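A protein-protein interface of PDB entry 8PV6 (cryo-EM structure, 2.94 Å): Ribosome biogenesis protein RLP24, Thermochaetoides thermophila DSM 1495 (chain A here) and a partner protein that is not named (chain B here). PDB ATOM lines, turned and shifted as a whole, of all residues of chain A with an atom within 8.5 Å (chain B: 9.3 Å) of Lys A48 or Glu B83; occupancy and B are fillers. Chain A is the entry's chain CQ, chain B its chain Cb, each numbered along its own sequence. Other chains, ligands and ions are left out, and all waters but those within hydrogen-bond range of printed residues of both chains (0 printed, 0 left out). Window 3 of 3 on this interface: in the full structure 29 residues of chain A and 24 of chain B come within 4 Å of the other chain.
The guanidinium group (NH2) of Arg A47 sits at hydrogen-bond distance from the backbone carbonyl oxygen (O) of Gly B84.
The guanidinium group (NH2) of Arg A47 lies within hydrogen-bond range of the backbone carbonyl oxygen (O) of Ala B85 (3.4 Å).
OE2 of Glu B90 is in salt-bridge range of NE of Arg A47 (2.5 Å).
The side-chain amino group of Lys A48 lies within salt-bridge range of the side-chain carboxylate of Glu B83.
The backbone NH of Arg A47 lies within hydrogen-bond range of the side-chain amide oxygen of Asn A45 (2.9 Å).
The backbone carbonyl oxygen (O) of Pro A46 lies within hydrogen-bond range of the side-chain hydroxyl (OG1) of Thr A52, at 2.4 Å.
The side-chain carboxylate (OE2) of Glu B23 sits at hydrogen-bond distance from the backbone NH (N) of Ala B85 (2.5 Å).
Tyr B86 touches Phe A8 (OH to O, 3.6 Å).
Tyr B86 touches Asn A45.
Pro A46 touches Tyr B86.
Arg A47 touches Tyr B86.
CB of Ala A54 touches CE1 of Tyr B86, at 3.5 Å.
Of chain A, only Lys A48 (3.4 Å) comes within 4 Å of Glu B83.
Gly B84 touches just one residue of chain A: Arg A47.
Of the printed residues of chain A, Glu B90 touches Arg A47.
Printed residues of chain B within 4 Å of Pro A46: Tyr B86 (3.6 Å).
The nearest residue of chain B that does not touch Lys A48 is Lys B79 (5.9 Å).
The nearest residue of chain A that does not touch Glu B83 is Arg A47 (4.2 Å).
The nearest printed residue of chain A that does not touch Ala B85 is Asn A45 (5.3 Å).
Of the 15 printed residues of chain B, 5 touch a printed residue of chain A.
Printed residues of chain B that touch a printed residue of chain A: Glu B83, Gly B84, Ala B85, Tyr B86 and Glu B90.
Of the 14 printed residues of chain A, 6 touch a printed residue of chain B.
Printed residues of chain A that touch a printed residue of chain B: Phe A8, Asn A45, Pro A46, Arg A47, Lys A48 and Ala A54.
Among the printed residues, Asp or Glu carboxylates within 4 Å of a Lys or Arg side-chain nitrogen of the other chain: Arg A47 with Glu B90 and Lys A48 with Glu B83.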
ATOM      1  N   PHE A   8     -18.891  24.586  -8.780  1.00  0.00           N
ATOM      2  CA  PHE A   8     -18.118  24.569  -7.547  1.00  0.00           C
ATOM      3  C   PHE A   8     -17.509  23.200  -7.275  1.00  0.00           C
ATOM      4  O   PHE A   8     -16.283  23.062  -7.219  1.00  0.00           O
ATOM      5  CB  PHE A   8     -19.001  24.994  -6.376  1.00  0.00           C
ATOM      6  CG  PHE A   8     -18.236  25.502  -5.196  1.00  0.00           C
ATOM      7  CD1 PHE A   8     -17.941  26.848  -5.077  1.00  0.00           C
ATOM      8  CD2 PHE A   8     -17.805  24.634  -4.208  1.00  0.00           C
ATOM      9  CE1 PHE A   8     -17.236  27.320  -3.992  1.00  0.00           C
ATOM     10  CE2 PHE A   8     -17.097  25.099  -3.124  1.00  0.00           C
ATOM     11  CZ  PHE A   8     -16.809  26.443  -3.019  1.00  0.00           C
ATOM     12  N   ARG A  44     -15.422  31.384  -1.131  1.00  0.00           N
ATOM     13  CA  ARG A  44     -14.520  30.301  -0.775  1.00  0.00           C
ATOM     14  C   ARG A  44     -14.013  29.618  -2.038  1.00  0.00           C
ATOM     15  O   ARG A  44     -14.763  29.423  -2.998  1.00  0.00           O
ATOM     16  CB  ARG A  44     -15.222  29.290   0.130  1.00  0.00           C
ATOM     17  CG  ARG A  44     -15.888  29.911   1.340  1.00  0.00           C
ATOM     18  CD  ARG A  44     -15.772  29.009   2.551  1.00  0.00           C
ATOM     19  NE  ARG A  44     -14.385  28.836   2.965  1.00  0.00           N
ATOM     20  CZ  ARG A  44     -13.998  28.084   3.985  1.00  0.00           C
ATOM     21  NH1 ARG A  44     -14.869  27.411   4.716  1.00  0.00           N
ATOM     22  NH2 ARG A  44     -12.703  28.003   4.276  1.00  0.00           N
ATOM     23  N   ASN A  45     -12.737  29.267  -2.035  1.00  0.00           N
ATOM     24  CA  ASN A  45     -12.129  28.658  -3.212  1.00  0.00           C
ATOM     25  C   ASN A  45     -12.471  27.173  -3.267  1.00  0.00           C
ATOM     26  O   ASN A  45     -12.252  26.458  -2.284  1.00  0.00           O
ATOM     27  CB  ASN A  45     -10.616  28.849  -3.190  1.00  0.00           C
ATOM     28  CG  ASN A  45      -9.996  28.775  -4.570  1.00  0.00           C
ATOM     29  OD1 ASN A  45     -10.294  27.876  -5.352  1.00  0.00           O
ATOM     30  ND2 ASN A  45      -9.127  29.730  -4.878  1.00  0.00           N
ATOM     31  N   PRO A  46     -13.024  26.681  -4.379  1.00  0.00           N
ATOM     32  CA  PRO A  46     -13.245  25.232  -4.511  1.00  0.00           C
ATOM     33  C   PRO A  46     -11.965  24.418  -4.514  1.00  0.00           C
ATOM     34  O   PRO A  46     -11.997  23.229  -4.174  1.00  0.00           O
ATOM     35  CB  PRO A  46     -13.987  25.109  -5.849  1.00  0.00           C
ATOM     36  CG  PRO A  46     -14.522  26.463  -6.130  1.00  0.00           C
ATOM     37  CD  PRO A  46     -13.563  27.430  -5.525  1.00  0.00           C
ATOM     38  N   ARG A  47     -10.837  25.021  -4.894  1.00  0.00           N
ATOM     39  CA  ARG A  47      -9.569  24.307  -4.922  1.00  0.00           C
ATOM     40  C   ARG A  47      -9.007  24.048  -3.532  1.00  0.00           C
ATOM     41  O   ARG A  47      -8.086  23.237  -3.395  1.00  0.00           O
ATOM     42  CB  ARG A  47      -8.556  25.088  -5.761  1.00  0.00           C
ATOM     43  CG  ARG A  47      -7.488  24.233  -6.414  1.00  0.00           C
ATOM     44  CD  ARG A  47      -6.390  25.076  -7.044  1.00  0.00           C
ATOM     45  NE  ARG A  47      -6.896  25.988  -8.062  1.00  0.00           N
ATOM     46  CZ  ARG A  47      -6.919  27.308  -7.941  1.00  0.00           C
ATOM     47  NH1 ARG A  47      -6.473  27.910  -6.851  1.00  0.00           N
ATOM     48  NH2 ARG A  47      -7.398  28.043  -8.940  1.00  0.00           N
ATOM     49  N   LYS A  48      -9.538  24.705  -2.499  1.00  0.00           N
ATOM     50  CA  LYS A  48      -9.054  24.520  -1.141  1.00  0.00           C
ATOM     51  C   LYS A  48     -10.014  23.754  -0.246  1.00  0.00           C
ATOM     52  O   LYS A  48      -9.597  23.296   0.822  1.00  0.00           O
ATOM     53  CB  LYS A  48      -8.745  25.879  -0.497  1.00  0.00           C
ATOM     54  CG  LYS A  48      -7.558  26.588  -1.121  1.00  0.00           C
ATOM     55  CD  LYS A  48      -6.784  27.380  -0.088  1.00  0.00           C
ATOM     56  CE  LYS A  48      -5.426  27.798  -0.620  1.00  0.00           C
ATOM     57  NZ  LYS A  48      -4.606  28.463   0.429  1.00  0.00           N
ATOM     58  N   LEU A  49     -11.275  23.604  -0.644  1.00  0.00           N
ATOM     59  CA  LEU A  49     -12.224  22.798   0.114  1.00  0.00           C
ATOM     60  C   LEU A  49     -12.085  21.341  -0.309  1.00  0.00           C
ATOM     61  O   LEU A  49     -12.248  21.014  -1.487  1.00  0.00           O
ATOM     62  CB  LEU A  49     -13.647  23.304  -0.105  1.00  0.00           C
ATOM     63  CG  LEU A  49     -13.868  24.794   0.163  1.00  0.00           C
ATOM     64  CD1 LEU A  49     -15.329  25.155   0.023  1.00  0.00           C
ATOM     65  CD2 LEU A  49     -13.366  25.176   1.541  1.00  0.00           C
ATOM     66  N   LYS A  50     -11.805  20.465   0.658  1.00  0.00           N
ATOM     67  CA  LYS A  50     -11.350  19.111   0.362  1.00  0.00           C
ATOM     68  C   LYS A  50     -12.441  18.192  -0.173  1.00  0.00           C
ATOM     69  O   LYS A  50     -12.122  17.084  -0.612  1.00  0.00           O
ATOM     70  CB  LYS A  50     -10.725  18.482   1.606  1.00  0.00           C
ATOM     71  CG  LYS A  50      -9.644  19.323   2.250  1.00  0.00           C
ATOM     72  CD  LYS A  50      -9.045  18.615   3.449  1.00  0.00           C
ATOM     73  CE  LYS A  50      -7.832  19.357   3.981  1.00  0.00           C
ATOM     74  NZ  LYS A  50      -7.197  18.635   5.116  1.00  0.00           N
ATOM     75  N   TRP A  51     -13.701  18.608  -0.150  1.00  0.00           N
ATOM     76  CA  TRP A  51     -14.791  17.776  -0.637  1.00  0.00           C
ATOM     77  C   TRP A  51     -15.126  18.042  -2.099  1.00  0.00           C
ATOM     78  O   TRP A  51     -16.179  17.601  -2.569  1.00  0.00           O
ATOM     79  CB  TRP A  51     -16.038  17.975   0.231  1.00  0.00           C
ATOM     80  CG  TRP A  51     -16.413  19.410   0.444  1.00  0.00           C
ATOM     81  CD1 TRP A  51     -15.941  20.245   1.413  1.00  0.00           C
ATOM     82  CD2 TRP A  51     -17.344  20.175  -0.325  1.00  0.00           C
ATOM     83  NE1 TRP A  51     -16.516  21.484   1.291  1.00  0.00           N
ATOM     84  CE2 TRP A  51     -17.383  21.467   0.230  1.00  0.00           C
ATOM     85  CE3 TRP A  51     -18.149  19.894  -1.432  1.00  0.00           C
ATOM     86  CZ2 TRP A  51     -18.191  22.476  -0.284  1.00  0.00           C
ATOM     87  CZ3 TRP A  51     -18.950  20.897  -1.940  1.00  0.00           C
ATOM     88  CH2 TRP A  51     -18.967  22.170  -1.366  1.00  0.00           C
ATOM     89  N   THR A  52     -14.262  18.742  -2.825  1.00  0.00           N
ATOM     90  CA  THR A  52     -14.541  19.150  -4.193  1.00  0.00           C
ATOM     91  C   THR A  52     -13.588  18.477  -5.173  1.00  0.00           C
ATOM     92  O   THR A  52     -12.409  18.244  -4.872  1.00  0.00           O
ATOM     93  CB  THR A  52     -14.439  20.670  -4.348  1.00  0.00           C
ATOM     94  OG1 THR A  52     -13.098  21.093  -4.074  1.00  0.00           O
ATOM     95  CG2 THR A  52     -15.389  21.370  -3.395  1.00  0.00           C
ATOM     96  N   ALA A  54     -12.325  19.834  -7.692  1.00  0.00           N
ATOM     97  CA  ALA A  54     -11.222  20.754  -7.949  1.00  0.00           C
ATOM     98  C   ALA A  54     -10.046  20.476  -7.024  1.00  0.00           C
ATOM     99  O   ALA A  54      -8.895  20.393  -7.472  1.00  0.00           O
ATOM    100  CB  ALA A  54     -11.700  22.193  -7.785  1.00  0.00           C
ATOM    101  N   TYR A  55     -10.321  20.310  -5.725  1.00  0.00           N
ATOM    102  CA  TYR A  55      -9.261  19.967  -4.782  1.00  0.00           C
ATOM    103  C   TYR A  55      -8.671  18.603  -5.091  1.00  0.00           C
ATOM    104  O   TYR A  55      -7.454  18.419  -5.001  1.00  0.00           O
ATOM    105  CB  TYR A  55      -9.779  19.992  -3.342  1.00  0.00           C
ATOM    106  CG  TYR A  55      -8.790  19.437  -2.325  1.00  0.00           C
ATOM    107  CD1 TYR A  55      -8.854  18.110  -1.898  1.00  0.00           C
ATOM    108  CD2 TYR A  55      -7.791  20.242  -1.798  1.00  0.00           C
ATOM    109  CE1 TYR A  55      -7.953  17.610  -0.984  1.00  0.00           C
ATOM    110  CE2 TYR A  55      -6.887  19.747  -0.878  1.00  0.00           C
ATOM    111  CZ  TYR A  55      -6.973  18.431  -0.476  1.00  0.00           C
ATOM    112  OH  TYR A  55      -6.077  17.933   0.439  1.00  0.00           O
ATOM    113  N   ARG A  56      -9.519  17.623  -5.410  1.00  0.00           N
ATOM    114  CA  ARG A  56      -9.002  16.277  -5.634  1.00  0.00           C
ATOM    115  C   ARG A  56      -8.150  16.206  -6.901  1.00  0.00           C
ATOM    116  O   ARG A  56      -7.129  15.508  -6.932  1.00  0.00           O
ATOM    117  CB  ARG A  56     -10.154  15.278  -5.675  1.00  0.00           C
ATOM    118  CG  ARG A  56     -11.073  15.358  -4.473  1.00  0.00           C
ATOM    119  CD  ARG A  56     -12.101  14.243  -4.460  1.00  0.00           C
ATOM    120  NE  ARG A  56     -11.690  13.136  -3.605  1.00  0.00           N
ATOM    121  CZ  ARG A  56     -11.186  11.994  -4.049  1.00  0.00           C
ATOM    122  NH1 ARG A  56     -11.038  11.760  -5.342  1.00  0.00           N
ATOM    123  NH2 ARG A  56     -10.827  11.060  -3.173  1.00  0.00           N
ATOM    124  N   ASN A  58      -6.470  18.858  -8.074  1.00  0.00           N
ATOM    125  CA  ASN A  58      -5.261  19.615  -7.766  1.00  0.00           C
ATOM    126  C   ASN A  58      -4.295  18.809  -6.910  1.00  0.00           C
ATOM    127  O   ASN A  58      -3.075  18.959  -7.043  1.00  0.00           O
ATOM    128  CB  ASN A  58      -5.624  20.921  -7.065  1.00  0.00           C
ATOM    129  CG  ASN A  58      -4.447  21.863  -6.947  1.00  0.00           C
ATOM    130  OD1 ASN A  58      -3.621  21.957  -7.852  1.00  0.00           O
ATOM    131  ND2 ASN A  58      -4.361  22.565  -5.826  1.00  0.00           N
ATOM    132  N   LEU B  19     -12.455  37.317  -8.187  1.00  0.00           N
ATOM    133  CA  LEU B  19     -11.019  37.207  -8.423  1.00  0.00           C
ATOM    134  C   LEU B  19     -10.693  36.907  -9.880  1.00  0.00           C
ATOM    135  O   LEU B  19      -9.660  37.359 -10.384  1.00  0.00           O
ATOM    136  CB  LEU B  19     -10.426  36.131  -7.516  1.00  0.00           C
ATOM    137  CG  LEU B  19      -8.923  36.213  -7.260  1.00  0.00           C
ATOM    138  CD1 LEU B  19      -8.595  37.417  -6.396  1.00  0.00           C
ATOM    139  CD2 LEU B  19      -8.425  34.934  -6.615  1.00  0.00           C
ATOM    140  N   GLU B  23      -8.340  39.114 -12.258  1.00  0.00           N
ATOM    141  CA  GLU B  23      -7.287  38.629 -13.151  1.00  0.00           C
ATOM    142  C   GLU B  23      -7.474  39.134 -14.575  1.00  0.00           C
ATOM    143  O   GLU B  23      -6.495  39.464 -15.253  1.00  0.00           O
ATOM    144  CB  GLU B  23      -7.218  37.104 -13.153  1.00  0.00           C
ATOM    145  CG  GLU B  23      -6.764  36.482 -11.862  1.00  0.00           C
ATOM    146  CD  GLU B  23      -6.734  34.972 -11.941  1.00  0.00           C
ATOM    147  OE1 GLU B  23      -7.190  34.422 -12.965  1.00  0.00           O
ATOM    148  OE2 GLU B  23      -6.228  34.337 -10.995  1.00  0.00           O
ATOM    149  N   LYS B  75      -2.118  41.704   0.824  1.00  0.00           N
ATOM    150  CA  LYS B  75      -1.212  40.570   0.672  1.00  0.00           C
ATOM    151  C   LYS B  75      -1.966  39.256   0.496  1.00  0.00           C
ATOM    152  O   LYS B  75      -1.479  38.350  -0.193  1.00  0.00           O
ATOM    153  CB  LYS B  75      -0.268  40.500   1.869  1.00  0.00           C
ATOM    154  CG  LYS B  75       0.709  41.660   1.921  1.00  0.00           C
ATOM    155  CD  LYS B  75       1.651  41.554   3.100  1.00  0.00           C
ATOM    156  CE  LYS B  75       2.601  42.736   3.140  1.00  0.00           C
ATOM    157  NZ  LYS B  75       3.528  42.655   4.299  1.00  0.00           N
ATOM    158  N   ARG B  76      -3.149  39.132   1.100  1.00  0.00           N
ATOM    159  CA  ARG B  76      -3.997  37.981   0.813  1.00  0.00           C
ATOM    160  C   ARG B  76      -4.460  38.002  -0.635  1.00  0.00           C
ATOM    161  O   ARG B  76      -4.528  36.954  -1.284  1.00  0.00           O
ATOM    162  CB  ARG B  76      -5.198  37.934   1.760  1.00  0.00           C
ATOM    163  CG  ARG B  76      -6.046  36.683   1.561  1.00  0.00           C
ATOM    164  CD  ARG B  76      -7.238  36.585   2.489  1.00  0.00           C
ATOM    165  NE  ARG B  76      -8.240  37.609   2.233  1.00  0.00           N
ATOM    166  CZ  ARG B  76      -9.287  37.832   3.015  1.00  0.00           C
ATOM    167  NH1 ARG B  76      -9.539  37.069   4.064  1.00  0.00           N
ATOM    168  NH2 ARG B  76     -10.111  38.836   2.725  1.00  0.00           N
ATOM    169  N   ARG B  77      -4.772  39.188  -1.161  1.00  0.00           N
ATOM    170  CA  ARG B  77      -5.091  39.291  -2.581  1.00  0.00           C
ATOM    171  C   ARG B  77      -3.886  38.935  -3.447  1.00  0.00           C
ATOM    172  O   ARG B  77      -4.042  38.307  -4.500  1.00  0.00           O
ATOM    173  CB  ARG B  77      -5.606  40.692  -2.901  1.00  0.00           C
ATOM    174  CG  ARG B  77      -7.099  40.829  -2.673  1.00  0.00           C
ATOM    175  CD  ARG B  77      -7.874  39.931  -3.623  1.00  0.00           C
ATOM    176  NE  ARG B  77      -9.265  39.760  -3.219  1.00  0.00           N
ATOM    177  CZ  ARG B  77     -10.233  40.631  -3.465  1.00  0.00           C
ATOM    178  NH1 ARG B  77      -9.998  41.764  -4.104  1.00  0.00           N
ATOM    179  NH2 ARG B  77     -11.469  40.359  -3.057  1.00  0.00           N
ATOM    180  N   LEU B  78      -2.677  39.315  -3.007  1.00  0.00           N
ATOM    181  CA  LEU B  78      -1.452  38.905  -3.698  1.00  0.00           C
ATOM    182  C   LEU B  78      -1.334  37.391  -3.769  1.00  0.00           C
ATOM    183  O   LEU B  78      -1.073  36.831  -4.839  1.00  0.00           O
ATOM    184  CB  LEU B  78      -0.207  39.461  -2.999  1.00  0.00           C
ATOM    185  CG  LEU B  78       0.095  40.944  -2.806  1.00  0.00           C
ATOM    186  CD1 LEU B  78       1.590  41.157  -2.638  1.00  0.00           C
ATOM    187  CD2 LEU B  78      -0.407  41.727  -3.970  1.00  0.00           C
ATOM    188  N   LYS B  79      -1.532  36.713  -2.637  1.00  0.00           N
ATOM    189  CA  LYS B  79      -1.356  35.265  -2.615  1.00  0.00           C
ATOM    190  C   LYS B  79      -2.479  34.556  -3.371  1.00  0.00           C
ATOM    191  O   LYS B  79      -2.244  33.526  -4.012  1.00  0.00           O
ATOM    192  CB  LYS B  79      -1.229  34.765  -1.169  1.00  0.00           C
ATOM    193  CG  LYS B  79      -2.524  34.529  -0.407  1.00  0.00           C
ATOM    194  CD  LYS B  79      -2.277  33.817   0.913  1.00  0.00           C
ATOM    195  CE  LYS B  79      -3.414  34.070   1.892  1.00  0.00           C
ATOM    196  NZ  LYS B  79      -3.083  33.623   3.273  1.00  0.00           N
ATOM    197  N   GLN B  80      -3.690  35.123  -3.362  1.00  0.00           N
ATOM    198  CA  GLN B  80      -4.790  34.521  -4.109  1.00  0.00           C
ATOM    199  C   GLN B  80      -4.585  34.675  -5.610  1.00  0.00           C
ATOM    200  O   GLN B  80      -4.863  33.748  -6.378  1.00  0.00           O
ATOM    201  CB  GLN B  80      -6.121  35.135  -3.678  1.00  0.00           C
ATOM    202  CG  GLN B  80      -6.600  34.684  -2.309  1.00  0.00           C
ATOM    203  CD  GLN B  80      -7.865  35.392  -1.870  1.00  0.00           C
ATOM    204  OE1 GLN B  80      -8.366  36.278  -2.559  1.00  0.00           O
ATOM    205  NE2 GLN B  80      -8.385  35.006  -0.712  1.00  0.00           N
ATOM    206  N   LEU B  81      -4.087  35.836  -6.046  1.00  0.00           N
ATOM    207  CA  LEU B  81      -3.770  36.015  -7.458  1.00  0.00           C
ATOM    208  C   LEU B  81      -2.577  35.167  -7.878  1.00  0.00           C
ATOM    209  O   LEU B  81      -2.515  34.717  -9.027  1.00  0.00           O
ATOM    210  CB  LEU B  81      -3.499  37.489  -7.755  1.00  0.00           C
ATOM    211  CG  LEU B  81      -4.692  38.441  -7.686  1.00  0.00           C
ATOM    212  CD1 LEU B  81      -4.215  39.874  -7.525  1.00  0.00           C
ATOM    213  CD2 LEU B  81      -5.568  38.309  -8.912  1.00  0.00           C
ATOM    214  N   LYS B  82      -1.619  34.954  -6.974  1.00  0.00           N
ATOM    215  CA  LYS B  82      -0.476  34.104  -7.286  1.00  0.00           C
ATOM    216  C   LYS B  82      -0.899  32.649  -7.442  1.00  0.00           C
ATOM    217  O   LYS B  82      -0.425  31.948  -8.343  1.00  0.00           O
ATOM    218  CB  LYS B  82       0.589  34.247  -6.200  1.00  0.00           C
ATOM    219  CG  LYS B  82       1.800  33.354  -6.387  1.00  0.00           C
ATOM    220  CD  LYS B  82       2.464  33.040  -5.059  1.00  0.00           C
ATOM    221  CE  LYS B  82       3.153  34.267  -4.489  1.00  0.00           C
ATOM    222  NZ  LYS B  82       3.971  34.973  -5.512  1.00  0.00           N
ATOM    223  N   GLU B  83      -1.791  32.176  -6.567  1.00  0.00           N
ATOM    224  CA  GLU B  83      -2.329  30.829  -6.726  1.00  0.00           C
ATOM    225  C   GLU B  83      -3.187  30.721  -7.980  1.00  0.00           C
ATOM    226  O   GLU B  83      -3.147  29.705  -8.682  1.00  0.00           O
ATOM    227  CB  GLU B  83      -3.128  30.429  -5.488  1.00  0.00           C
ATOM    228  CG  GLU B  83      -2.287  30.260  -4.239  1.00  0.00           C
ATOM    229  CD  GLU B  83      -3.114  29.883  -3.030  1.00  0.00           C
ATOM    230  OE1 GLU B  83      -4.358  29.875  -3.139  1.00  0.00           O
ATOM    231  OE2 GLU B  83      -2.522  29.597  -1.970  1.00  0.00           O
ATOM    232  N   GLY B  84      -3.954  31.755  -8.284  1.00  0.00           N
ATOM    233  CA  GLY B  84      -4.784  31.766  -9.478  1.00  0.00           C
ATOM    234  C   GLY B  84      -6.248  31.589  -9.125  1.00  0.00           C
ATOM    235  O   GLY B  84      -6.610  30.770  -8.272  1.00  0.00           O
ATOM    236  N   ALA B  85      -7.103  32.364  -9.785  1.00  0.00           N
ATOM    237  CA  ALA B  85      -8.530  32.262  -9.533  1.00  0.00           C
ATOM    238  C   ALA B  85      -9.107  31.001 -10.171  1.00  0.00           C
ATOM    239  O   ALA B  85      -8.545  30.424 -11.106  1.00  0.00           O
ATOM    240  CB  ALA B  85      -9.265  33.494 -10.057  1.00  0.00           C
ATOM    241  N   TYR B  86     -10.250  30.580  -9.642  1.00  0.00           N
ATOM    242  CA  TYR B  86     -10.934  29.382 -10.099  1.00  0.00           C
ATOM    243  C   TYR B  86     -11.893  29.743 -11.226  1.00  0.00           C
ATOM    244  O   TYR B  86     -12.745  30.622 -11.065  1.00  0.00           O
ATOM    245  CB  TYR B  86     -11.683  28.744  -8.931  1.00  0.00           C
ATOM    246  CG  TYR B  86     -12.394  27.466  -9.267  1.00  0.00           C
ATOM    247  CD1 TYR B  86     -11.703  26.271  -9.352  1.00  0.00           C
ATOM    248  CD2 TYR B  86     -13.763  27.451  -9.482  1.00  0.00           C
ATOM    249  CE1 TYR B  86     -12.353  25.099  -9.654  1.00  0.00           C
ATOM    250  CE2 TYR B  86     -14.422  26.282  -9.781  1.00  0.00           C
ATOM    251  CZ  TYR B  86     -13.713  25.108  -9.864  1.00  0.00           C
ATOM    252  OH  TYR B  86     -14.369  23.939 -10.159  1.00  0.00           O
ATOM    253  N   GLU B  90     -10.860  25.426 -15.399  1.00  0.00           N
ATOM    254  CA  GLU B  90     -10.381  24.628 -14.277  1.00  0.00           C
ATOM    255  C   GLU B  90     -11.477  23.700 -13.764  1.00  0.00           C
ATOM    256  O   GLU B  90     -11.203  22.553 -13.388  1.00  0.00           O
ATOM    257  CB  GLU B  90      -9.873  25.547 -13.165  1.00  0.00           C
ATOM    258  CG  GLU B  90      -9.512  24.845 -11.869  1.00  0.00           C
ATOM    259  CD  GLU B  90      -8.348  25.503 -11.162  1.00  0.00           C
ATOM    260  OE1 GLU B  90      -7.846  26.528 -11.669  1.00  0.00           O
ATOM    261  OE2 GLU B  90      -7.933  24.997 -10.099  1.00  0.00           O
